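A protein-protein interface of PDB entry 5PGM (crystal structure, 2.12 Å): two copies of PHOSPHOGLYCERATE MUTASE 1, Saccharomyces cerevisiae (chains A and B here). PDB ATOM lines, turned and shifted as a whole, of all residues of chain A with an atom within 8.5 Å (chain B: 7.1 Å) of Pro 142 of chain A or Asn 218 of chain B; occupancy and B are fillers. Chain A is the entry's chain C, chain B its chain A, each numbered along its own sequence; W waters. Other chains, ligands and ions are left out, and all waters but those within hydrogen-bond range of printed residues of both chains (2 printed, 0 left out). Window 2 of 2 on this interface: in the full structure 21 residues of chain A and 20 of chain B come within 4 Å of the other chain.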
ATOM      1  N   LYS A 132      18.458  33.826  14.873  1.00  0.00           N
ATOM      2  CA  LYS A 132      19.196  33.714  16.121  1.00  0.00           C
ATOM      3  C   LYS A 132      18.512  34.414  17.305  1.00  0.00           C
ATOM      4  O   LYS A 132      18.327  35.633  17.293  1.00  0.00           O
ATOM      5  CB  LYS A 132      20.619  34.244  15.927  1.00  0.00           C
ATOM      6  CG  LYS A 132      21.673  33.602  16.826  1.00  0.00           C
ATOM      7  CD  LYS A 132      21.996  34.434  18.054  1.00  0.00           C
ATOM      8  CE  LYS A 132      23.089  33.760  18.913  1.00  0.00           C
ATOM      9  NZ  LYS A 132      22.717  32.390  19.456  1.00  0.00           N
ATOM     10  N   GLY A 133      18.159  33.659  18.343  1.00  0.00           N
ATOM     11  CA  GLY A 133      17.529  34.314  19.487  1.00  0.00           C
ATOM     12  C   GLY A 133      16.003  34.356  19.419  1.00  0.00           C
ATOM     13  O   GLY A 133      15.362  34.965  20.293  1.00  0.00           O
ATOM     14  N   TYR A 137      12.606  29.013  19.649  1.00  0.00           N
ATOM     15  CA  TYR A 137      13.736  28.101  19.795  1.00  0.00           C
ATOM     16  C   TYR A 137      14.472  28.361  21.123  1.00  0.00           C
ATOM     17  O   TYR A 137      15.561  27.828  21.313  1.00  0.00           O
ATOM     18  CB  TYR A 137      14.737  28.230  18.622  1.00  0.00           C
ATOM     19  CG  TYR A 137      14.166  28.125  17.209  1.00  0.00           C
ATOM     20  CD1 TYR A 137      13.543  26.952  16.774  1.00  0.00           C
ATOM     21  CD2 TYR A 137      14.187  29.240  16.331  1.00  0.00           C
ATOM     22  CE1 TYR A 137      12.931  26.870  15.497  1.00  0.00           C
ATOM     23  CE2 TYR A 137      13.577  29.170  15.049  1.00  0.00           C
ATOM     24  CZ  TYR A 137      12.962  27.987  14.652  1.00  0.00           C
ATOM     25  OH  TYR A 137      12.404  27.857  13.409  1.00  0.00           O
ATOM     26  N   LYS A 138      13.863  29.128  22.039  1.00  0.00           N
ATOM     27  CA  LYS A 138      14.471  29.482  23.326  1.00  0.00           C
ATOM     28  C   LYS A 138      14.732  28.327  24.321  1.00  0.00           C
ATOM     29  O   LYS A 138      15.479  28.510  25.291  1.00  0.00           O
ATOM     30  CB  LYS A 138      13.699  30.617  24.039  1.00  0.00           C
ATOM     31  CG  LYS A 138      12.297  30.240  24.604  1.00  0.00           C
ATOM     32  CD  LYS A 138      11.776  31.413  25.438  1.00  0.00           C
ATOM     33  CE  LYS A 138      10.595  31.035  26.376  1.00  0.00           C
ATOM     34  NZ  LYS A 138      10.696  31.740  27.745  1.00  0.00           N
ATOM     35  N   TYR A 139      14.122  27.168  24.076  1.00  0.00           N
ATOM     36  CA  TYR A 139      14.304  26.009  24.962  1.00  0.00           C
ATOM     37  C   TYR A 139      15.203  24.922  24.323  1.00  0.00           C
ATOM     38  O   TYR A 139      15.283  23.790  24.821  1.00  0.00           O
ATOM     39  CB  TYR A 139      12.939  25.428  25.387  1.00  0.00           C
ATOM     40  CG  TYR A 139      12.124  26.311  26.340  1.00  0.00           C
ATOM     41  CD1 TYR A 139      12.699  26.849  27.498  1.00  0.00           C
ATOM     42  CD2 TYR A 139      10.778  26.609  26.079  1.00  0.00           C
ATOM     43  CE1 TYR A 139      11.971  27.653  28.373  1.00  0.00           C
ATOM     44  CE2 TYR A 139      10.030  27.420  26.956  1.00  0.00           C
ATOM     45  CZ  TYR A 139      10.638  27.935  28.101  1.00  0.00           C
ATOM     46  OH  TYR A 139       9.914  28.692  28.997  1.00  0.00           O
ATOM     47  N   VAL A 140      15.777  25.246  23.159  1.00  0.00           N
ATOM     48  CA  VAL A 140      16.684  24.355  22.445  1.00  0.00           C
ATOM     49  C   VAL A 140      18.106  24.813  22.821  1.00  0.00           C
ATOM     50  O   VAL A 140      18.319  25.969  23.167  1.00  0.00           O
ATOM     51  CB  VAL A 140      16.490  24.445  20.911  1.00  0.00           C
ATOM     52  CG1 VAL A 140      17.475  23.472  20.186  1.00  0.00           C
ATOM     53  CG2 VAL A 140      15.068  24.083  20.540  1.00  0.00           C
ATOM     54  N   ASP A 141      19.057  23.890  22.860  1.00  0.00           N
ATOM     55  CA  ASP A 141      20.429  24.250  23.190  1.00  0.00           C
ATOM     56  C   ASP A 141      20.821  25.278  22.122  1.00  0.00           C
ATOM     57  O   ASP A 141      20.762  25.002  20.926  1.00  0.00           O
ATOM     58  CB  ASP A 141      21.289  22.974  23.087  1.00  0.00           C
ATOM     59  CG  ASP A 141      22.774  23.248  23.107  1.00  0.00           C
ATOM     60  OD1 ASP A 141      23.270  24.315  23.524  1.00  0.00           O
ATOM     61  OD2 ASP A 141      23.478  22.356  22.667  1.00  0.00           O
ATOM     62  N   PRO A 142      21.188  26.487  22.538  1.00  0.00           N
ATOM     63  CA  PRO A 142      21.568  27.498  21.556  1.00  0.00           C
ATOM     64  C   PRO A 142      22.670  27.057  20.594  1.00  0.00           C
ATOM     65  O   PRO A 142      22.720  27.528  19.468  1.00  0.00           O
ATOM     66  CB  PRO A 142      22.101  28.637  22.419  1.00  0.00           C
ATOM     67  CG  PRO A 142      21.362  28.474  23.721  1.00  0.00           C
ATOM     68  CD  PRO A 142      21.346  26.985  23.917  1.00  0.00           C
ATOM     69  N   ASN A 143      23.554  26.164  21.055  1.00  0.00           N
ATOM     70  CA  ASN A 143      24.724  25.751  20.264  1.00  0.00           C
ATOM     71  C   ASN A 143      24.453  24.911  19.036  1.00  0.00           C
ATOM     72  O   ASN A 143      25.229  24.957  18.095  1.00  0.00           O
ATOM     73  CB  ASN A 143      25.750  25.027  21.155  1.00  0.00           C
ATOM     74  CG  ASN A 143      26.153  25.840  22.356  1.00  0.00           C
ATOM     75  OD1 ASN A 143      27.009  26.710  22.253  1.00  0.00           O
ATOM     76  ND2 ASN A 143      25.507  25.587  23.510  1.00  0.00           N
ATOM     77  N   VAL A 144      23.355  24.154  19.056  1.00  0.00           N
ATOM     78  CA  VAL A 144      23.019  23.281  17.944  1.00  0.00           C
ATOM     79  C   VAL A 144      22.266  23.962  16.814  1.00  0.00           C
ATOM     80  O   VAL A 144      22.211  23.443  15.686  1.00  0.00           O
ATOM     81  CB  VAL A 144      22.173  22.127  18.401  1.00  0.00           C
ATOM     82  CG1 VAL A 144      20.811  22.590  18.804  1.00  0.00           C
ATOM     83  CG2 VAL A 144      22.022  21.149  17.324  1.00  0.00           C
ATOM     84  N   LEU A 145      21.642  25.088  17.136  1.00  0.00           N
ATOM     85  CA  LEU A 145      20.840  25.818  16.161  1.00  0.00           C
ATOM     86  C   LEU A 145      21.739  26.352  15.038  1.00  0.00           C
ATOM     87  O   LEU A 145      22.591  27.205  15.265  1.00  0.00           O
ATOM     88  CB  LEU A 145      20.049  26.912  16.884  1.00  0.00           C
ATOM     89  CG  LEU A 145      18.604  26.758  17.365  1.00  0.00           C
ATOM     90  CD1 LEU A 145      18.003  25.422  17.200  1.00  0.00           C
ATOM     91  CD2 LEU A 145      18.501  27.319  18.752  1.00  0.00           C
ATOM     92  N   PRO A 146      21.457  25.950  13.796  1.00  0.00           N
ATOM     93  CA  PRO A 146      22.218  26.324  12.600  1.00  0.00           C
ATOM     94  C   PRO A 146      22.114  27.735  12.074  1.00  0.00           C
ATOM     95  O   PRO A 146      21.060  28.325  12.159  1.00  0.00           O
ATOM     96  CB  PRO A 146      21.696  25.336  11.574  1.00  0.00           C
ATOM     97  CG  PRO A 146      20.249  25.292  11.903  1.00  0.00           C
ATOM     98  CD  PRO A 146      20.273  25.154  13.415  1.00  0.00           C
ATOM     99  N   GLU A 147      23.208  28.245  11.489  1.00  0.00           N
ATOM    100  CA  GLU A 147      23.251  29.570  10.879  1.00  0.00           C
ATOM    101  C   GLU A 147      23.382  29.463   9.364  1.00  0.00           C
ATOM    102  O   GLU A 147      23.453  30.448   8.634  1.00  0.00           O
ATOM    103  CB  GLU A 147      24.303  30.422  11.525  1.00  0.00           C
ATOM    104  CG  GLU A 147      23.811  30.784  12.889  1.00  0.00           C
ATOM    105  CD  GLU A 147      24.672  31.813  13.581  1.00  0.00           C
ATOM    106  OE1 GLU A 147      25.676  31.399  14.227  1.00  0.00           O
ATOM    107  OE2 GLU A 147      24.348  33.031  13.502  1.00  0.00           O
ATOM    108  N   PRO B   1      21.966  27.847  34.949  1.00  0.00           N
ATOM    109  CA  PRO B   1      21.390  26.499  35.139  1.00  0.00           C
ATOM    110  C   PRO B   1      22.410  25.652  35.893  1.00  0.00           C
ATOM    111  O   PRO B   1      23.604  25.953  35.866  1.00  0.00           O
ATOM    112  CB  PRO B   1      21.134  25.924  33.753  1.00  0.00           C
ATOM    113  CG  PRO B   1      20.987  27.194  32.926  1.00  0.00           C
ATOM    114  CD  PRO B   1      21.901  28.222  33.525  1.00  0.00           C
ATOM    115  N   TRP B 162      20.463  15.627  24.696  1.00  0.00           N
ATOM    116  CA  TRP B 162      20.922  16.712  25.514  1.00  0.00           C
ATOM    117  C   TRP B 162      20.369  18.018  24.959  1.00  0.00           C
ATOM    118  O   TRP B 162      19.914  18.888  25.702  1.00  0.00           O
ATOM    119  CB  TRP B 162      22.445  16.741  25.512  1.00  0.00           C
ATOM    120  CG  TRP B 162      23.071  18.047  25.915  1.00  0.00           C
ATOM    121  CD1 TRP B 162      23.567  18.980  25.079  1.00  0.00           C
ATOM    122  CD2 TRP B 162      23.264  18.558  27.244  1.00  0.00           C
ATOM    123  NE1 TRP B 162      24.066  20.043  25.799  1.00  0.00           N
ATOM    124  CE2 TRP B 162      23.878  19.801  27.132  1.00  0.00           C
ATOM    125  CE3 TRP B 162      22.956  18.075  28.542  1.00  0.00           C
ATOM    126  CZ2 TRP B 162      24.192  20.585  28.245  1.00  0.00           C
ATOM    127  CZ3 TRP B 162      23.272  18.853  29.630  1.00  0.00           C
ATOM    128  CH2 TRP B 162      23.883  20.090  29.473  1.00  0.00           C
ATOM    129  N   GLN B 163      20.389  18.117  23.634  1.00  0.00           N
ATOM    130  CA  GLN B 163      20.003  19.325  22.925  1.00  0.00           C
ATOM    131  C   GLN B 163      18.579  19.784  23.035  1.00  0.00           C
ATOM    132  O   GLN B 163      18.333  20.968  23.148  1.00  0.00           O
ATOM    133  CB  GLN B 163      20.390  19.160  21.455  1.00  0.00           C
ATOM    134  CG  GLN B 163      21.920  19.315  21.286  1.00  0.00           C
ATOM    135  CD  GLN B 163      22.462  18.779  19.949  1.00  0.00           C
ATOM    136  OE1 GLN B 163      21.748  18.088  19.179  1.00  0.00           O
ATOM    137  NE2 GLN B 163      23.744  19.047  19.699  1.00  0.00           N
ATOM    138  N   ALA B 167      18.205  20.049  27.752  1.00  0.00           N
ATOM    139  CA  ALA B 167      18.359  21.516  27.617  1.00  0.00           C
ATOM    140  C   ALA B 167      17.102  22.315  27.997  1.00  0.00           C
ATOM    141  O   ALA B 167      17.200  23.401  28.548  1.00  0.00           O
ATOM    142  CB  ALA B 167      18.775  21.873  26.140  1.00  0.00           C
ATOM    143  N   LEU B 171      17.238  25.219  30.646  1.00  0.00           N
ATOM    144  CA  LEU B 171      16.843  26.555  30.195  1.00  0.00           C
ATOM    145  C   LEU B 171      15.521  27.028  30.880  1.00  0.00           C
ATOM    146  O   LEU B 171      15.204  28.218  30.883  1.00  0.00           O
ATOM    147  CB  LEU B 171      16.756  26.571  28.654  1.00  0.00           C
ATOM    148  CG  LEU B 171      18.141  26.364  27.994  1.00  0.00           C
ATOM    149  CD1 LEU B 171      18.026  26.058  26.566  1.00  0.00           C
ATOM    150  CD2 LEU B 171      18.993  27.580  28.203  1.00  0.00           C
ATOM    151  N   LEU B 215      26.215  26.256  34.702  1.00  0.00           N
ATOM    152  CA  LEU B 215      26.180  26.676  33.306  1.00  0.00           C
ATOM    153  C   LEU B 215      25.555  28.055  33.072  1.00  0.00           C
ATOM    154  O   LEU B 215      24.767  28.525  33.893  1.00  0.00           O
ATOM    155  CB  LEU B 215      25.391  25.633  32.509  1.00  0.00           C
ATOM    156  CG  LEU B 215      25.856  24.180  32.645  1.00  0.00           C
ATOM    157  CD1 LEU B 215      24.910  23.203  31.905  1.00  0.00           C
ATOM    158  CD2 LEU B 215      27.306  23.998  32.165  1.00  0.00           C
ATOM    159  N   ASP B 216      25.924  28.711  31.969  1.00  0.00           N
ATOM    160  CA  ASP B 216      25.343  29.995  31.616  1.00  0.00           C
ATOM    161  C   ASP B 216      24.182  29.753  30.639  1.00  0.00           C
ATOM    162  O   ASP B 216      23.844  28.600  30.360  1.00  0.00           O
ATOM    163  CB  ASP B 216      26.396  30.935  31.027  1.00  0.00           C
ATOM    164  CG  ASP B 216      26.955  30.464  29.681  1.00  0.00           C
ATOM    165  OD1 ASP B 216      26.414  29.544  29.018  1.00  0.00           O
ATOM    166  OD2 ASP B 216      27.966  31.059  29.286  1.00  0.00           O
ATOM    167  N   GLU B 217      23.577  30.810  30.098  1.00  0.00           N
ATOM    168  CA  GLU B 217      22.442  30.662  29.174  1.00  0.00           C
ATOM    169  C   GLU B 217      22.738  29.883  27.887  1.00  0.00           C
ATOM    170  O   GLU B 217      21.819  29.322  27.270  1.00  0.00           O
ATOM    171  CB  GLU B 217      21.782  32.021  28.861  1.00  0.00           C
ATOM    172  CG  GLU B 217      22.655  33.041  28.143  1.00  0.00           C
ATOM    173  CD  GLU B 217      23.737  33.682  29.019  1.00  0.00           C
ATOM    174  OE1 GLU B 217      23.904  33.307  30.220  1.00  0.00           O
ATOM    175  OE2 GLU B 217      24.441  34.592  28.489  1.00  0.00           O
ATOM    176  N   ASN B 218      24.027  29.785  27.522  1.00  0.00           N
ATOM    177  CA  ASN B 218      24.430  29.034  26.328  1.00  0.00           C
ATOM    178  C   ASN B 218      24.834  27.623  26.679  1.00  0.00           C
ATOM    179  O   ASN B 218      25.322  26.868  25.832  1.00  0.00           O
ATOM    180  CB  ASN B 218      25.557  29.781  25.606  1.00  0.00           C
ATOM    181  CG  ASN B 218      25.087  31.144  25.078  1.00  0.00           C
ATOM    182  OD1 ASN B 218      24.083  31.216  24.390  1.00  0.00           O
ATOM    183  ND2 ASN B 218      25.764  32.210  25.456  1.00  0.00           N
ATOM    184  N   LEU B 219      24.528  27.247  27.927  1.00  0.00           N
ATOM    185  CA  LEU B 219      24.818  25.933  28.505  1.00  0.00           C
ATOM    186  C   LEU B 219      26.309  25.683  28.536  1.00  0.00           C
ATOM    187  O   LEU B 219      26.779  24.565  28.366  1.00  0.00           O
ATOM    188  CB  LEU B 219      24.071  24.810  27.784  1.00  0.00           C
ATOM    189  CG  LEU B 219      22.562  25.009  27.778  1.00  0.00           C
ATOM    190  CD1 LEU B 219      21.904  23.836  27.090  1.00  0.00           C
ATOM    191  CD2 LEU B 219      22.054  25.163  29.221  1.00  0.00           C
ATOM    192  N   LYS B 220      27.045  26.740  28.813  1.00  0.00           N
ATOM    193  CA  LYS B 220      28.481  26.629  28.871  1.00  0.00           C
ATOM    194  C   LYS B 220      28.987  26.857  30.297  1.00  0.00           C
ATOM    195  O   LYS B 220      28.489  27.721  31.007  1.00  0.00           O
ATOM    196  CB  LYS B 220      29.104  27.590  27.843  1.00  0.00           C
ATOM    197  CG  LYS B 220      30.494  28.105  28.229  1.00  0.00           C
ATOM    198  CD  LYS B 220      31.252  28.807  27.094  1.00  0.00           C
ATOM    199  CE  LYS B 220      32.484  29.564  27.644  1.00  0.00           C
ATOM    200  NZ  LYS B 220      33.428  30.015  26.565  1.00  0.00           N
ATOM    201  N   PRO B 221      29.971  26.068  30.751  1.00  0.00           N
ATOM    202  CA  PRO B 221      30.460  26.282  32.111  1.00  0.00           C
ATOM    203  C   PRO B 221      30.728  27.731  32.464  1.00  0.00           C
ATOM    204  O   PRO B 221      31.444  28.407  31.741  1.00  0.00           O
ATOM    205  CB  PRO B 221      31.741  25.453  32.139  1.00  0.00           C
ATOM    206  CG  PRO B 221      31.371  24.263  31.326  1.00  0.00           C
ATOM    207  CD  PRO B 221      30.606  24.881  30.141  1.00  0.00           C
HETATM  208  O   HOH W   1      25.622  22.358  24.550  1.00  0.00           O
HETATM  209  O   HOH W   2      25.068  20.782  21.132  1.00  0.00           O
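NZ of Lys 138 of chain A lies within hydrogen-bond range of OH of Tyr 139 of chain A, 3.4 Å away. The side-chain carboxylate (OD1) of Asp 141 of chain A is in hydrogen-bond range of the side-chain amide nitrogen (ND2) of Asn 143 of chain A, at 2.6 Å. The backbone NH (N) of Ala 167 of chain B is in hydrogen-bond range of the backbone carbonyl oxygen (O) of Trp 162 of chain B (2.9 Å). N of Asn 218 of chain B is in hydrogen-bond range of OD1 of Asp 216 of chain B (2.8 Å). The side-chain carboxylate of Asp 216 of chain B is in hydrogen-bond range of the backbone NH of Leu 219 of chain B (3.2 Å).
Lys 138 of chain A touches Leu 171 of chain B (O to CD1, 3.8 Å). Ala 167 of chain B touches Tyr 139 of chain A. CD1 of Leu 171 of chain B touches C of Tyr 139 of chain A, at 3.8 Å. Val 140 of chain A touches Gln 163 of chain B. Val 140 of chain A touches Leu 171 of chain B. Asp 141 of chain A touches Trp 162 of chain B (OD2 to NE1, 3.9 Å). N of Asp 141 of chain A touches CB of Ala 167 of chain B, 3.9 Å away. Asp 141 of chain A touches Leu 219 of chain B. CB of Pro 142 of chain A touches OD1 of Asn 218 of chain B, 3.8 Å away. Val 144 of chain A touches Gln 163 of chain B (CG2 to CD, 3.6 Å).
The backbone NH of Asp 141 of chain A is in hydrogen-bond range of the backbone carbonyl oxygen of Gln 163 of chain B (3.0 Å). The backbone carbonyl oxygen of Asn 218 of chain B lies within hydrogen-bond range of the side-chain amide nitrogen of Asn 143 of chain A, at 2.7 Å.
Water W2 lies within hydrogen-bond range of NE2 of Gln 163 of chain B and OD2 of Asp 141 of chain A. Water W1 lies within hydrogen-bond range of OD2 of Asp 141 of chain A (2.9 Å), NE1 of Trp 162 of chain B (3.1 Å) and ND2 of Asn 143 of chain A (3.4 Å).
Printed residues of chain B that touch a printed residue of chain A: Trp 162, Gln 163, Ala 167, Leu 171, Glu 217, Asn 218 and Leu 219. Hydrophobic or aromatic side chains of chain B that line the printed part of chain A: Trp 162, Ala 167, Leu 171 and Leu 219. Printed residues of chain A that touch a printed residue of chain B: Lys 138, Tyr 139, Val 140, Asp 141, Pro 142, Asn 143 and Val 144. Hydrophobic or aromatic side chains of chain A within 4 Å of the printed part of chain B: Val 140, Pro 142 and Val 144. Among the printed residues, 13 pairs touch across the chains.
Printed residues of chain B within 4 Å of Pro 142 of chain A: Glu 217 and Asn 218. Of chain A, only Pro 142 comes within 4 Å of Glu 217 of chain B. Of the printed residues of chain B, Lys 138 of chain A touches Leu 171 (3.8 Å). Printed residues of chain A within 4 Å of Leu 219 of chain B: Asp 141 (3.8 Å). Printed residues of chain A within 4 Å of Ala 167 of chain B: Tyr 139 and Asp 141. Of the printed residues of chain B, Tyr 139 of chain A touches Ala 167 (3.9 Å) and Leu 171 (3.8 Å). Leu 145 of chain A touches none of the printed residues of chain B. The nearest residue of chain B that does not touch Pro 142 of chain A is Leu 171 of chain B (4.3 Å). The nearest printed residue of chain A that does not touch Ala 167 of chain B is Val 140 of chain A (4.5 Å).
No position is printed for both chains.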
